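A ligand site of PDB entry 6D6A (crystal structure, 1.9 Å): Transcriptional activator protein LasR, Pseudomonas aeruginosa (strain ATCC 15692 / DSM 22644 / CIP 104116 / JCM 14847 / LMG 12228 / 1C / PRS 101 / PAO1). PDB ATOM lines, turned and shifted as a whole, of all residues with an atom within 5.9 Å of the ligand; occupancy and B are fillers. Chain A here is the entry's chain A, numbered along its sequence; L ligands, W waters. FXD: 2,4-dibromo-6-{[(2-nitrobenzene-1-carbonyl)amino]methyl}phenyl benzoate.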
ATOM      1  N   LEU A  36     -17.088 -34.486 -32.729  1.00  0.00           N
ATOM      2  CA  LEU A  36     -15.895 -33.661 -32.695  1.00  0.00           C
ATOM      3  C   LEU A  36     -15.060 -34.107 -31.477  1.00  0.00           C
ATOM      4  O   LEU A  36     -15.592 -34.171 -30.339  1.00  0.00           O
ATOM      5  CB  LEU A  36     -16.221 -32.166 -32.661  1.00  0.00           C
ATOM      6  CG  LEU A  36     -14.923 -31.275 -32.684  1.00  0.00           C
ATOM      7  CD1 LEU A  36     -15.125 -29.952 -33.404  1.00  0.00           C
ATOM      8  CD2 LEU A  36     -14.447 -30.949 -31.255  1.00  0.00           C
ATOM      9  N   PHE A  37     -13.798 -34.427 -31.755  1.00  0.00           N
ATOM     10  CA  PHE A  37     -12.773 -34.758 -30.781  1.00  0.00           C
ATOM     11  C   PHE A  37     -11.785 -33.621 -30.820  1.00  0.00           C
ATOM     12  O   PHE A  37     -11.217 -33.302 -31.883  1.00  0.00           O
ATOM     13  CB  PHE A  37     -12.105 -36.078 -31.178  1.00  0.00           C
ATOM     14  CG  PHE A  37     -10.956 -36.472 -30.298  1.00  0.00           C
ATOM     15  CD1 PHE A  37      -9.663 -36.037 -30.579  1.00  0.00           C
ATOM     16  CD2 PHE A  37     -11.161 -37.266 -29.158  1.00  0.00           C
ATOM     17  CE1 PHE A  37      -8.571 -36.392 -29.752  1.00  0.00           C
ATOM     18  CE2 PHE A  37     -10.070 -37.651 -28.351  1.00  0.00           C
ATOM     19  CZ  PHE A  37      -8.788 -37.205 -28.649  1.00  0.00           C
ATOM     20  N   GLY A  38     -11.668 -32.911 -29.705  1.00  0.00           N
ATOM     21  CA  GLY A  38     -10.892 -31.677 -29.583  1.00  0.00           C
ATOM     22  C   GLY A  38      -9.893 -31.865 -28.414  1.00  0.00           C
ATOM     23  O   GLY A  38     -10.266 -32.361 -27.293  1.00  0.00           O
ATOM     24  N   LEU A  39      -8.660 -31.431 -28.623  1.00  0.00           N
ATOM     25  CA  LEU A  39      -7.598 -31.660 -27.617  1.00  0.00           C
ATOM     26  C   LEU A  39      -6.528 -30.550 -27.625  1.00  0.00           C
ATOM     27  O   LEU A  39      -6.020 -30.162 -28.697  1.00  0.00           O
ATOM     28  CB  LEU A  39      -6.990 -33.007 -27.833  1.00  0.00           C
ATOM     29  CG  LEU A  39      -6.298 -33.601 -26.625  1.00  0.00           C
ATOM     30  CD1 LEU A  39      -7.371 -34.015 -25.607  1.00  0.00           C
ATOM     31  CD2 LEU A  39      -5.394 -34.767 -27.002  1.00  0.00           C
ATOM     32  N   LEU A  40      -6.270 -30.005 -26.450  1.00  0.00           N
ATOM     33  CA  LEU A  40      -5.222 -29.018 -26.209  1.00  0.00           C
ATOM     34  C   LEU A  40      -4.052 -29.591 -25.375  1.00  0.00           C
ATOM     35  O   LEU A  40      -4.286 -30.427 -24.481  1.00  0.00           O
ATOM     36  CB  LEU A  40      -5.809 -27.829 -25.474  1.00  0.00           C
ATOM     37  CG  LEU A  40      -6.758 -26.960 -26.267  1.00  0.00           C
ATOM     38  CD1 LEU A  40      -7.389 -25.990 -25.282  1.00  0.00           C
ATOM     39  CD2 LEU A  40      -5.934 -26.186 -27.324  1.00  0.00           C
ATOM     40  N   TYR A  47      -7.933 -22.355 -27.817  1.00  0.00           N
ATOM     41  CA  TYR A  47      -8.999 -23.219 -28.344  1.00  0.00           C
ATOM     42  C   TYR A  47      -9.046 -23.277 -29.858  1.00  0.00           C
ATOM     43  O   TYR A  47      -9.420 -24.325 -30.403  1.00  0.00           O
ATOM     44  CB  TYR A  47     -10.387 -22.863 -27.767  1.00  0.00           C
ATOM     45  CG  TYR A  47     -10.466 -23.095 -26.284  1.00  0.00           C
ATOM     46  CD1 TYR A  47     -10.675 -24.364 -25.773  1.00  0.00           C
ATOM     47  CD2 TYR A  47     -10.324 -22.037 -25.380  1.00  0.00           C
ATOM     48  CE1 TYR A  47     -10.682 -24.595 -24.397  1.00  0.00           C
ATOM     49  CE2 TYR A  47     -10.366 -22.242 -24.011  1.00  0.00           C
ATOM     50  CZ  TYR A  47     -10.543 -23.530 -23.512  1.00  0.00           C
ATOM     51  OH  TYR A  47     -10.560 -23.716 -22.140  1.00  0.00           O
ATOM     52  N   GLU A  48      -8.680 -22.179 -30.528  1.00  0.00           N
ATOM     53  CA  GLU A  48      -8.596 -22.136 -32.015  1.00  0.00           C
ATOM     54  C   GLU A  48      -7.406 -22.980 -32.588  1.00  0.00           C
ATOM     55  O   GLU A  48      -7.516 -23.462 -33.729  1.00  0.00           O
ATOM     56  CB  GLU A  48      -8.568 -20.681 -32.561  1.00  0.00           C
ATOM     57  CG  GLU A  48      -8.376 -20.580 -34.086  1.00  0.00           C
ATOM     58  CD  GLU A  48      -8.898 -19.291 -34.718  1.00  0.00           C
ATOM     59  OE1 GLU A  48     -10.122 -19.060 -34.691  1.00  0.00           O
ATOM     60  OE2 GLU A  48      -8.074 -18.528 -35.285  1.00  0.00           O
ATOM     61  N   ALA A  50      -6.540 -25.842 -31.239  1.00  0.00           N
ATOM     62  CA  ALA A  50      -6.726 -27.171 -30.699  1.00  0.00           C
ATOM     63  C   ALA A  50      -6.541 -28.197 -31.800  1.00  0.00           C
ATOM     64  O   ALA A  50      -6.853 -27.925 -32.943  1.00  0.00           O
ATOM     65  CB  ALA A  50      -8.112 -27.276 -30.083  1.00  0.00           C
ATOM     66  N   ILE A  52      -8.020 -30.995 -33.653  1.00  0.00           N
ATOM     67  CA  ILE A  52      -9.431 -31.305 -33.834  1.00  0.00           C
ATOM     68  C   ILE A  52      -9.614 -32.407 -34.844  1.00  0.00           C
ATOM     69  O   ILE A  52      -9.102 -32.317 -35.980  1.00  0.00           O
ATOM     70  CB  ILE A  52     -10.216 -30.043 -34.266  1.00  0.00           C
ATOM     71  CG1 ILE A  52     -10.262 -29.064 -33.073  1.00  0.00           C
ATOM     72  CG2 ILE A  52     -11.625 -30.424 -34.762  1.00  0.00           C
ATOM     73  CD1 ILE A  52     -10.795 -27.701 -33.420  1.00  0.00           C
ATOM     74  N   TYR A  56     -17.930 -32.773 -38.039  1.00  0.00           N
ATOM     75  CA  TYR A  56     -18.790 -31.567 -37.943  1.00  0.00           C
ATOM     76  C   TYR A  56     -18.700 -30.813 -39.295  1.00  0.00           C
ATOM     77  O   TYR A  56     -17.656 -30.841 -39.920  1.00  0.00           O
ATOM     78  CB  TYR A  56     -18.323 -30.647 -36.859  1.00  0.00           C
ATOM     79  CG  TYR A  56     -18.844 -30.936 -35.449  1.00  0.00           C
ATOM     80  CD1 TYR A  56     -19.423 -32.156 -35.091  1.00  0.00           C
ATOM     81  CD2 TYR A  56     -18.825 -29.937 -34.516  1.00  0.00           C
ATOM     82  CE1 TYR A  56     -19.875 -32.366 -33.792  1.00  0.00           C
ATOM     83  CE2 TYR A  56     -19.305 -30.125 -33.227  1.00  0.00           C
ATOM     84  CZ  TYR A  56     -19.807 -31.325 -32.863  1.00  0.00           C
ATOM     85  OH  TYR A  56     -20.230 -31.471 -31.556  1.00  0.00           O
ATOM     86  N   TRP A  60     -19.328 -24.804 -40.018  1.00  0.00           N
ATOM     87  CA  TRP A  60     -19.755 -24.599 -38.606  1.00  0.00           C
ATOM     88  C   TRP A  60     -18.494 -24.463 -37.768  1.00  0.00           C
ATOM     89  O   TRP A  60     -18.333 -23.519 -36.961  1.00  0.00           O
ATOM     90  CB  TRP A  60     -20.702 -25.717 -38.116  1.00  0.00           C
ATOM     91  CG  TRP A  60     -20.832 -25.715 -36.627  1.00  0.00           C
ATOM     92  CD1 TRP A  60     -20.396 -26.683 -35.794  1.00  0.00           C
ATOM     93  CD2 TRP A  60     -21.330 -24.669 -35.774  1.00  0.00           C
ATOM     94  NE1 TRP A  60     -20.630 -26.362 -34.487  1.00  0.00           N
ATOM     95  CE2 TRP A  60     -21.195 -25.128 -34.435  1.00  0.00           C
ATOM     96  CE3 TRP A  60     -21.885 -23.434 -36.002  1.00  0.00           C
ATOM     97  CZ2 TRP A  60     -21.620 -24.396 -33.329  1.00  0.00           C
ATOM     98  CZ3 TRP A  60     -22.296 -22.665 -34.885  1.00  0.00           C
ATOM     99  CH2 TRP A  60     -22.168 -23.166 -33.560  1.00  0.00           C
ATOM    100  N   ARG A  61     -17.546 -25.347 -37.997  1.00  0.00           N
ATOM    101  CA  ARG A  61     -16.220 -25.150 -37.383  1.00  0.00           C
ATOM    102  C   ARG A  61     -15.587 -23.825 -37.668  1.00  0.00           C
ATOM    103  O   ARG A  61     -15.023 -23.229 -36.755  1.00  0.00           O
ATOM    104  CB  ARG A  61     -15.247 -26.279 -37.703  1.00  0.00           C
ATOM    105  CG  ARG A  61     -15.708 -27.601 -37.121  1.00  0.00           C
ATOM    106  CD  ARG A  61     -15.009 -28.768 -37.758  1.00  0.00           C
ATOM    107  NE  ARG A  61     -13.631 -28.712 -37.373  1.00  0.00           N
ATOM    108  CZ  ARG A  61     -12.599 -29.029 -38.152  1.00  0.00           C
ATOM    109  NH1 ARG A  61     -12.777 -29.445 -39.421  1.00  0.00           N
ATOM    110  NH2 ARG A  61     -11.365 -28.912 -37.659  1.00  0.00           N
ATOM    111  N   TYR A  64     -17.500 -21.159 -35.674  1.00  0.00           N
ATOM    112  CA  TYR A  64     -17.142 -21.244 -34.214  1.00  0.00           C
ATOM    113  C   TYR A  64     -15.860 -20.511 -33.915  1.00  0.00           C
ATOM    114  O   TYR A  64     -15.806 -19.757 -32.947  1.00  0.00           O
ATOM    115  CB  TYR A  64     -16.993 -22.695 -33.831  1.00  0.00           C
ATOM    116  CG  TYR A  64     -16.921 -23.058 -32.353  1.00  0.00           C
ATOM    117  CD1 TYR A  64     -15.721 -22.952 -31.666  1.00  0.00           C
ATOM    118  CD2 TYR A  64     -18.003 -23.680 -31.719  1.00  0.00           C
ATOM    119  CE1 TYR A  64     -15.603 -23.342 -30.354  1.00  0.00           C
ATOM    120  CE2 TYR A  64     -17.896 -24.073 -30.364  1.00  0.00           C
ATOM    121  CZ  TYR A  64     -16.702 -23.883 -29.700  1.00  0.00           C
ATOM    122  OH  TYR A  64     -16.502 -24.255 -28.393  1.00  0.00           O
ATOM    123  N   ASP A  65     -14.841 -20.776 -34.717  1.00  0.00           N
ATOM    124  CA  ASP A  65     -13.522 -20.115 -34.632  1.00  0.00           C
ATOM    125  C   ASP A  65     -13.674 -18.616 -34.804  1.00  0.00           C
ATOM    126  O   ASP A  65     -13.301 -17.855 -33.912  1.00  0.00           O
ATOM    127  CB  ASP A  65     -12.559 -20.608 -35.711  1.00  0.00           C
ATOM    128  CG  ASP A  65     -11.750 -21.819 -35.297  1.00  0.00           C
ATOM    129  OD1 ASP A  65     -11.601 -22.119 -34.086  1.00  0.00           O
ATOM    130  OD2 ASP A  65     -11.237 -22.495 -36.225  1.00  0.00           O
ATOM    131  N   ALA A  70     -15.598 -20.577 -28.415  1.00  0.00           N
ATOM    132  CA  ALA A  70     -14.932 -21.249 -27.316  1.00  0.00           C
ATOM    133  C   ALA A  70     -15.100 -20.494 -25.982  1.00  0.00           C
ATOM    134  O   ALA A  70     -15.154 -21.110 -24.929  1.00  0.00           O
ATOM    135  CB  ALA A  70     -13.462 -21.468 -27.631  1.00  0.00           C
ATOM    136  N   ASP A  73     -19.676 -21.164 -25.656  1.00  0.00           N
ATOM    137  CA  ASP A  73     -20.071 -22.552 -25.589  1.00  0.00           C
ATOM    138  C   ASP A  73     -20.003 -23.031 -24.130  1.00  0.00           C
ATOM    139  O   ASP A  73     -18.899 -23.090 -23.563  1.00  0.00           O
ATOM    140  CB  ASP A  73     -19.055 -23.358 -26.465  1.00  0.00           C
ATOM    141  CG  ASP A  73     -19.292 -24.853 -26.460  1.00  0.00           C
ATOM    142  OD1 ASP A  73     -20.118 -25.393 -25.631  1.00  0.00           O
ATOM    143  OD2 ASP A  73     -18.677 -25.465 -27.380  1.00  0.00           O
ATOM    144  N   PRO A  74     -21.164 -23.370 -23.512  1.00  0.00           N
ATOM    145  CA  PRO A  74     -21.144 -23.743 -22.094  1.00  0.00           C
ATOM    146  C   PRO A  74     -20.452 -25.096 -21.832  1.00  0.00           C
ATOM    147  O   PRO A  74     -20.150 -25.421 -20.695  1.00  0.00           O
ATOM    148  CB  PRO A  74     -22.632 -23.866 -21.758  1.00  0.00           C
ATOM    149  CG  PRO A  74     -23.222 -24.289 -23.034  1.00  0.00           C
ATOM    150  CD  PRO A  74     -22.542 -23.402 -24.039  1.00  0.00           C
ATOM    151  N   THR A  75     -20.276 -25.921 -22.859  1.00  0.00           N
ATOM    152  CA  THR A  75     -19.628 -27.184 -22.633  1.00  0.00           C
ATOM    153  C   THR A  75     -18.145 -26.962 -22.408  1.00  0.00           C
ATOM    154  O   THR A  75     -17.483 -27.792 -21.761  1.00  0.00           O
ATOM    155  CB  THR A  75     -19.816 -28.230 -23.751  1.00  0.00           C
ATOM    156  OG1 THR A  75     -19.193 -27.770 -24.932  1.00  0.00           O
ATOM    157  CG2 THR A  75     -21.308 -28.546 -23.976  1.00  0.00           C
ATOM    158  N   VAL A  76     -17.623 -25.870 -22.942  1.00  0.00           N
ATOM    159  CA  VAL A  76     -16.207 -25.580 -22.746  1.00  0.00           C
ATOM    160  C   VAL A  76     -15.866 -25.225 -21.298  1.00  0.00           C
ATOM    161  O   VAL A  76     -14.956 -25.853 -20.712  1.00  0.00           O
ATOM    162  CB  VAL A  76     -15.650 -24.532 -23.751  1.00  0.00           C
ATOM    163  CG1 VAL A  76     -14.151 -24.242 -23.493  1.00  0.00           C
ATOM    164  CG2 VAL A  76     -15.790 -25.072 -25.177  1.00  0.00           C
ATOM    165  N   CYS A  79     -16.037 -28.485 -19.295  1.00  0.00           N
ATOM    166  CA  CYS A  79     -14.889 -29.337 -19.468  1.00  0.00           C
ATOM    167  C   CYS A  79     -13.695 -28.917 -18.582  1.00  0.00           C
ATOM    168  O   CYS A  79     -12.940 -29.751 -18.176  1.00  0.00           O
ATOM    169  CB  CYS A  79     -14.408 -29.379 -20.936  1.00  0.00           C
ATOM    170  SG  CYS A  79     -15.506 -30.411 -21.947  1.00  0.00           S
ATOM    171  N   TRP A  88     -26.592 -31.803 -23.944  1.00  0.00           N
ATOM    172  CA  TRP A  88     -27.002 -30.564 -24.588  1.00  0.00           C
ATOM    173  C   TRP A  88     -28.469 -30.139 -24.307  1.00  0.00           C
ATOM    174  O   TRP A  88     -29.255 -29.917 -25.216  1.00  0.00           O
ATOM    175  CB  TRP A  88     -26.735 -30.598 -26.086  1.00  0.00           C
ATOM    176  CG  TRP A  88     -25.302 -30.904 -26.492  1.00  0.00           C
ATOM    177  CD1 TRP A  88     -24.213 -30.995 -25.709  1.00  0.00           C
ATOM    178  CD2 TRP A  88     -24.846 -31.187 -27.828  1.00  0.00           C
ATOM    179  NE1 TRP A  88     -23.104 -31.324 -26.461  1.00  0.00           N
ATOM    180  CE2 TRP A  88     -23.461 -31.429 -27.765  1.00  0.00           C
ATOM    181  CE3 TRP A  88     -25.480 -31.201 -29.069  1.00  0.00           C
ATOM    182  CZ2 TRP A  88     -22.686 -31.712 -28.901  1.00  0.00           C
ATOM    183  CZ3 TRP A  88     -24.744 -31.499 -30.184  1.00  0.00           C
ATOM    184  CH2 TRP A  88     -23.344 -31.770 -30.101  1.00  0.00           C
ATOM    185  N   ILE A  92     -28.574 -25.618 -20.266  1.00  0.00           N
ATOM    186  CA  ILE A  92     -27.147 -25.189 -20.205  1.00  0.00           C
ATOM    187  C   ILE A  92     -26.864 -23.886 -20.908  1.00  0.00           C
ATOM    188  O   ILE A  92     -25.792 -23.354 -20.714  1.00  0.00           O
ATOM    189  CB  ILE A  92     -26.152 -26.283 -20.624  1.00  0.00           C
ATOM    190  CG1 ILE A  92     -26.197 -26.555 -22.140  1.00  0.00           C
ATOM    191  CG2 ILE A  92     -26.382 -27.451 -19.667  1.00  0.00           C
ATOM    192  CD1 ILE A  92     -25.101 -27.460 -22.699  1.00  0.00           C
ATOM    193  N   TYR A  93     -27.782 -23.418 -21.784  1.00  0.00           N
ATOM    194  CA  TYR A  93     -27.562 -22.172 -22.530  1.00  0.00           C
ATOM    195  C   TYR A  93     -28.210 -20.990 -21.745  1.00  0.00           C
ATOM    196  O   TYR A  93     -29.402 -20.850 -21.745  1.00  0.00           O
ATOM    197  CB  TYR A  93     -28.152 -22.346 -23.952  1.00  0.00           C
ATOM    198  CG  TYR A  93     -27.586 -23.561 -24.673  1.00  0.00           C
ATOM    199  CD1 TYR A  93     -26.278 -23.537 -25.199  1.00  0.00           C
ATOM    200  CD2 TYR A  93     -28.321 -24.749 -24.795  1.00  0.00           C
ATOM    201  CE1 TYR A  93     -25.748 -24.669 -25.853  1.00  0.00           C
ATOM    202  CE2 TYR A  93     -27.787 -25.847 -25.394  1.00  0.00           C
ATOM    203  CZ  TYR A  93     -26.515 -25.803 -25.952  1.00  0.00           C
ATOM    204  OH  TYR A  93     -26.024 -26.935 -26.545  1.00  0.00           O
ATOM    205  N   PHE A 101     -25.581 -19.079 -29.649  1.00  0.00           N
ATOM    206  CA  PHE A 101     -24.755 -20.254 -29.922  1.00  0.00           C
ATOM    207  C   PHE A 101     -25.679 -21.442 -30.060  1.00  0.00           C
ATOM    208  O   PHE A 101     -25.585 -22.139 -31.020  1.00  0.00           O
ATOM    209  CB  PHE A 101     -23.686 -20.449 -28.820  1.00  0.00           C
ATOM    210  CG  PHE A 101     -22.974 -21.766 -28.901  1.00  0.00           C
ATOM    211  CD1 PHE A 101     -21.903 -21.913 -29.722  1.00  0.00           C
ATOM    212  CD2 PHE A 101     -23.440 -22.885 -28.171  1.00  0.00           C
ATOM    213  CE1 PHE A 101     -21.247 -23.119 -29.842  1.00  0.00           C
ATOM    214  CE2 PHE A 101     -22.796 -24.100 -28.270  1.00  0.00           C
ATOM    215  CZ  PHE A 101     -21.704 -24.218 -29.116  1.00  0.00           C
ATOM    216  N   ALA A 105     -25.713 -23.462 -33.627  1.00  0.00           N
ATOM    217  CA  ALA A 105     -25.319 -24.864 -33.628  1.00  0.00           C
ATOM    218  C   ALA A 105     -26.465 -25.708 -34.210  1.00  0.00           C
ATOM    219  O   ALA A 105     -26.271 -26.650 -35.025  1.00  0.00           O
ATOM    220  CB  ALA A 105     -24.947 -25.321 -32.216  1.00  0.00           C
ATOM    221  N   LEU A 110     -26.568 -29.575 -35.275  1.00  0.00           N
ATOM    222  CA  LEU A 110     -26.014 -30.006 -33.977  1.00  0.00           C
ATOM    223  C   LEU A 110     -26.922 -29.486 -32.865  1.00  0.00           C
ATOM    224  O   LEU A 110     -26.731 -28.378 -32.348  1.00  0.00           O
ATOM    225  CB  LEU A 110     -24.563 -29.558 -33.816  1.00  0.00           C
ATOM    226  CG  LEU A 110     -23.665 -30.024 -35.015  1.00  0.00           C
ATOM    227  CD1 LEU A 110     -22.421 -29.150 -35.122  1.00  0.00           C
ATOM    228  CD2 LEU A 110     -23.390 -31.528 -34.970  1.00  0.00           C
ATOM    229  N   THR A 115     -21.346 -33.823 -24.588  1.00  0.00           N
ATOM    230  CA  THR A 115     -19.935 -33.570 -24.577  1.00  0.00           C
ATOM    231  C   THR A 115     -19.308 -34.332 -23.365  1.00  0.00           C
ATOM    232  O   THR A 115     -19.705 -34.107 -22.209  1.00  0.00           O
ATOM    233  CB  THR A 115     -19.651 -32.057 -24.486  1.00  0.00           C
ATOM    234  OG1 THR A 115     -20.178 -31.377 -25.656  1.00  0.00           O
ATOM    235  CG2 THR A 115     -18.133 -31.810 -24.407  1.00  0.00           C
ATOM    236  N   LEU A 125      -6.213 -31.323 -22.341  1.00  0.00           N
ATOM    237  CA  LEU A 125      -7.525 -30.837 -22.039  1.00  0.00           C
ATOM    238  C   LEU A 125      -8.289 -30.927 -23.309  1.00  0.00           C
ATOM    239  O   LEU A 125      -7.860 -30.381 -24.292  1.00  0.00           O
ATOM    240  CB  LEU A 125      -7.489 -29.397 -21.563  1.00  0.00           C
ATOM    241  CG  LEU A 125      -8.824 -28.621 -21.508  1.00  0.00           C
ATOM    242  CD1 LEU A 125      -9.750 -29.239 -20.488  1.00  0.00           C
ATOM    243  CD2 LEU A 125      -8.581 -27.155 -21.214  1.00  0.00           C
ATOM    244  N   GLY A 126      -9.452 -31.567 -23.270  1.00  0.00           N
ATOM    245  CA  GLY A 126     -10.260 -31.753 -24.429  1.00  0.00           C
ATOM    246  C   GLY A 126     -11.730 -32.055 -24.182  1.00  0.00           C
ATOM    247  O   GLY A 126     -12.243 -31.941 -23.058  1.00  0.00           O
ATOM    248  N   ALA A 127     -12.372 -32.412 -25.276  1.00  0.00           N
ATOM    249  CA  ALA A 127     -13.770 -32.687 -25.383  1.00  0.00           C
ATOM    250  C   ALA A 127     -13.991 -33.685 -26.499  1.00  0.00           C
ATOM    251  O   ALA A 127     -13.412 -33.521 -27.576  1.00  0.00           O
ATOM    252  CB  ALA A 127     -14.551 -31.375 -25.582  1.00  0.00           C
ATOM    253  N   SER A 129     -17.333 -34.432 -28.215  1.00  0.00           N
ATOM    254  CA  SER A 129     -18.739 -34.097 -28.489  1.00  0.00           C
ATOM    255  C   SER A 129     -19.323 -35.064 -29.509  1.00  0.00           C
ATOM    256  O   SER A 129     -18.679 -35.371 -30.528  1.00  0.00           O
ATOM    257  CB  SER A 129     -18.842 -32.682 -28.955  1.00  0.00           C
ATOM    258  OG  SER A 129     -18.518 -31.801 -27.863  1.00  0.00           O
HETATM  259  N16 FXD L   1     -21.240 -27.797 -31.265  1.00  0.00           N
HETATM  260  C15 FXD L   1     -21.729 -27.978 -29.982  1.00  0.00           C
HETATM  261  C2  FXD L   1     -14.278 -26.534 -30.659  1.00  0.00           C
HETATM  262  C1  FXD L   1     -15.003 -27.108 -29.631  1.00  0.00           C
HETATM  263  C10 FXD L   1     -20.877 -28.294 -28.934  1.00  0.00           C
HETATM  264  C9  FXD L   1     -19.423 -28.604 -29.140  1.00  0.00           C
HETATM  265  C12 FXD L   1     -22.786 -28.138 -27.397  1.00  0.00           C
HETATM  266  C14 FXD L   1     -23.091 -27.744 -29.731  1.00  0.00           C
HETATM  267  C7  FXD L   1     -17.068 -28.174 -28.658  1.00  0.00           C
HETATM  268  C6  FXD L   1     -16.327 -27.509 -29.794  1.00  0.00           C
HETATM  269  C5  FXD L   1     -16.940 -27.323 -31.042  1.00  0.00           C
HETATM  270  C4  FXD L   1     -16.218 -26.764 -32.053  1.00  0.00           C
HETATM  271  C3  FXD L   1     -14.910 -26.319 -31.872  1.00  0.00           C
HETATM  272  O17 FXD L   1     -19.242 -29.638 -29.804  1.00  0.00           O
HETATM  273  C11 FXD L   1     -21.415 -28.407 -27.630  1.00  0.00           C
HETATM  274  C13 FXD L   1     -23.622 -27.869 -28.454  1.00  0.00           C
HETATM  275  O18 FXD L   1     -22.004 -28.024 -32.338  1.00  0.00           O
HETATM  276  O19 FXD L   1     -19.990 -27.312 -31.479  1.00  0.00           O
HETATM  277  N8  FXD L   1     -18.499 -27.911 -28.579  1.00  0.00           N
HETATM  278 BR1  FXD L   1     -17.103 -26.485 -33.699  1.00  0.00          BR
HETATM  279 BR2  FXD L   1     -12.502 -25.847 -30.374  1.00  0.00          BR
HETATM  280  O20 FXD L   1     -14.408 -27.225 -28.410  1.00  0.00           O
HETATM  281  C21 FXD L   1     -13.362 -28.146 -28.174  1.00  0.00           C
HETATM  282  O22 FXD L   1     -13.074 -28.875 -29.055  1.00  0.00           O
HETATM  283  C25 FXD L   1     -12.696 -28.188 -26.851  1.00  0.00           C
HETATM  284  C30 FXD L   1     -13.461 -27.892 -25.743  1.00  0.00           C
HETATM  285  C29 FXD L   1     -12.929 -27.901 -24.474  1.00  0.00           C
HETATM  286  C26 FXD L   1     -11.363 -28.514 -26.756  1.00  0.00           C
HETATM  287  C27 FXD L   1     -10.806 -28.504 -25.484  1.00  0.00           C
HETATM  288  C28 FXD L   1     -11.579 -28.224 -24.338  1.00  0.00           C
HETATM  289  O   HOH W   1     -13.606 -24.798 -34.651  1.00  0.00           O
HETATM  290  O   HOH W   2     -16.605 -28.694 -24.635  1.00  0.00           O
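Residues that only touch the ligand: Leu 36 (3.3 Å), Gly 38 (3.6 Å), Tyr 47 (3.4 Å), Ile 52 (3.95 Å), Arg 61 (3.9 Å), Tyr 64 (3.4 Å), Thr 75 (3.6 Å), Val 76 (3.7 Å), Trp 88 (3.3 Å), Tyr 93 (3.2 Å), Phe 101 (3.8 Å), Ala 105 (3.9 Å), Leu 110 (3.0 Å), Thr 115 (3.8 Å), Leu 125 (3.7 Å), Gly 126 (3.5 Å) and Ala 127 (3.7 Å). The nearest printed residue that does not touch the ligand is Cys 79 (4.1 Å).
The side-chain carboxylate (OD2) of Asp 73 lies within hydrogen-bond range of the side-chain hydroxyl (OH) of Tyr 64. The backbone NH (N) of Ser 129 sits at hydrogen-bond distance from the backbone carbonyl oxygen (O) of Leu 36. OG of Ser 129 is in hydrogen-bond range of OG1 of Thr 115. The backbone NH (N) of Leu 110 is in hydrogen-bond range of the backbone carbonyl oxygen (O) of Ala 105, at 3.0 Å. NE1 of Trp 88 is in hydrogen-bond range of OG1 of Thr 115, at 3.0 Å. The backbone carbonyl oxygen of Gly 126 sits at hydrogen-bond distance from the side-chain sulfur of Cys 79, at 3.8 Å. O of Thr 75 is in hydrogen-bond range of SG of Cys 79 (3.3 Å). The backbone carbonyl oxygen (O) of Leu 125 lies within hydrogen-bond range of the backbone NH (N) of Leu 40 (2.7 Å).
Water W1 lies within hydrogen-bond range of O of Arg 61 (3.0 Å) and OD1 of Asp 65 (3.4 Å). Water W2 lies within hydrogen-bond range of the side-chain hydroxyl of Thr 75, the side-chain sulfur of Cys 79 and the backbone NH of Val 76.
O17 of the ligand sits at hydrogen-bond distance from OH of Tyr 56 (2.7 Å). The side-chain carboxylate of Asp 73 sits at hydrogen-bond distance from a nitrogen (N8) of the ligand (2.7 Å). An oxygen (O17) of the ligand sits at hydrogen-bond distance from the side-chain hydroxyl (OG) of Ser 129. The indole nitrogen of Trp 60 sits at hydrogen-bond distance from an oxygen (O18) of the ligand (3.0 Å).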
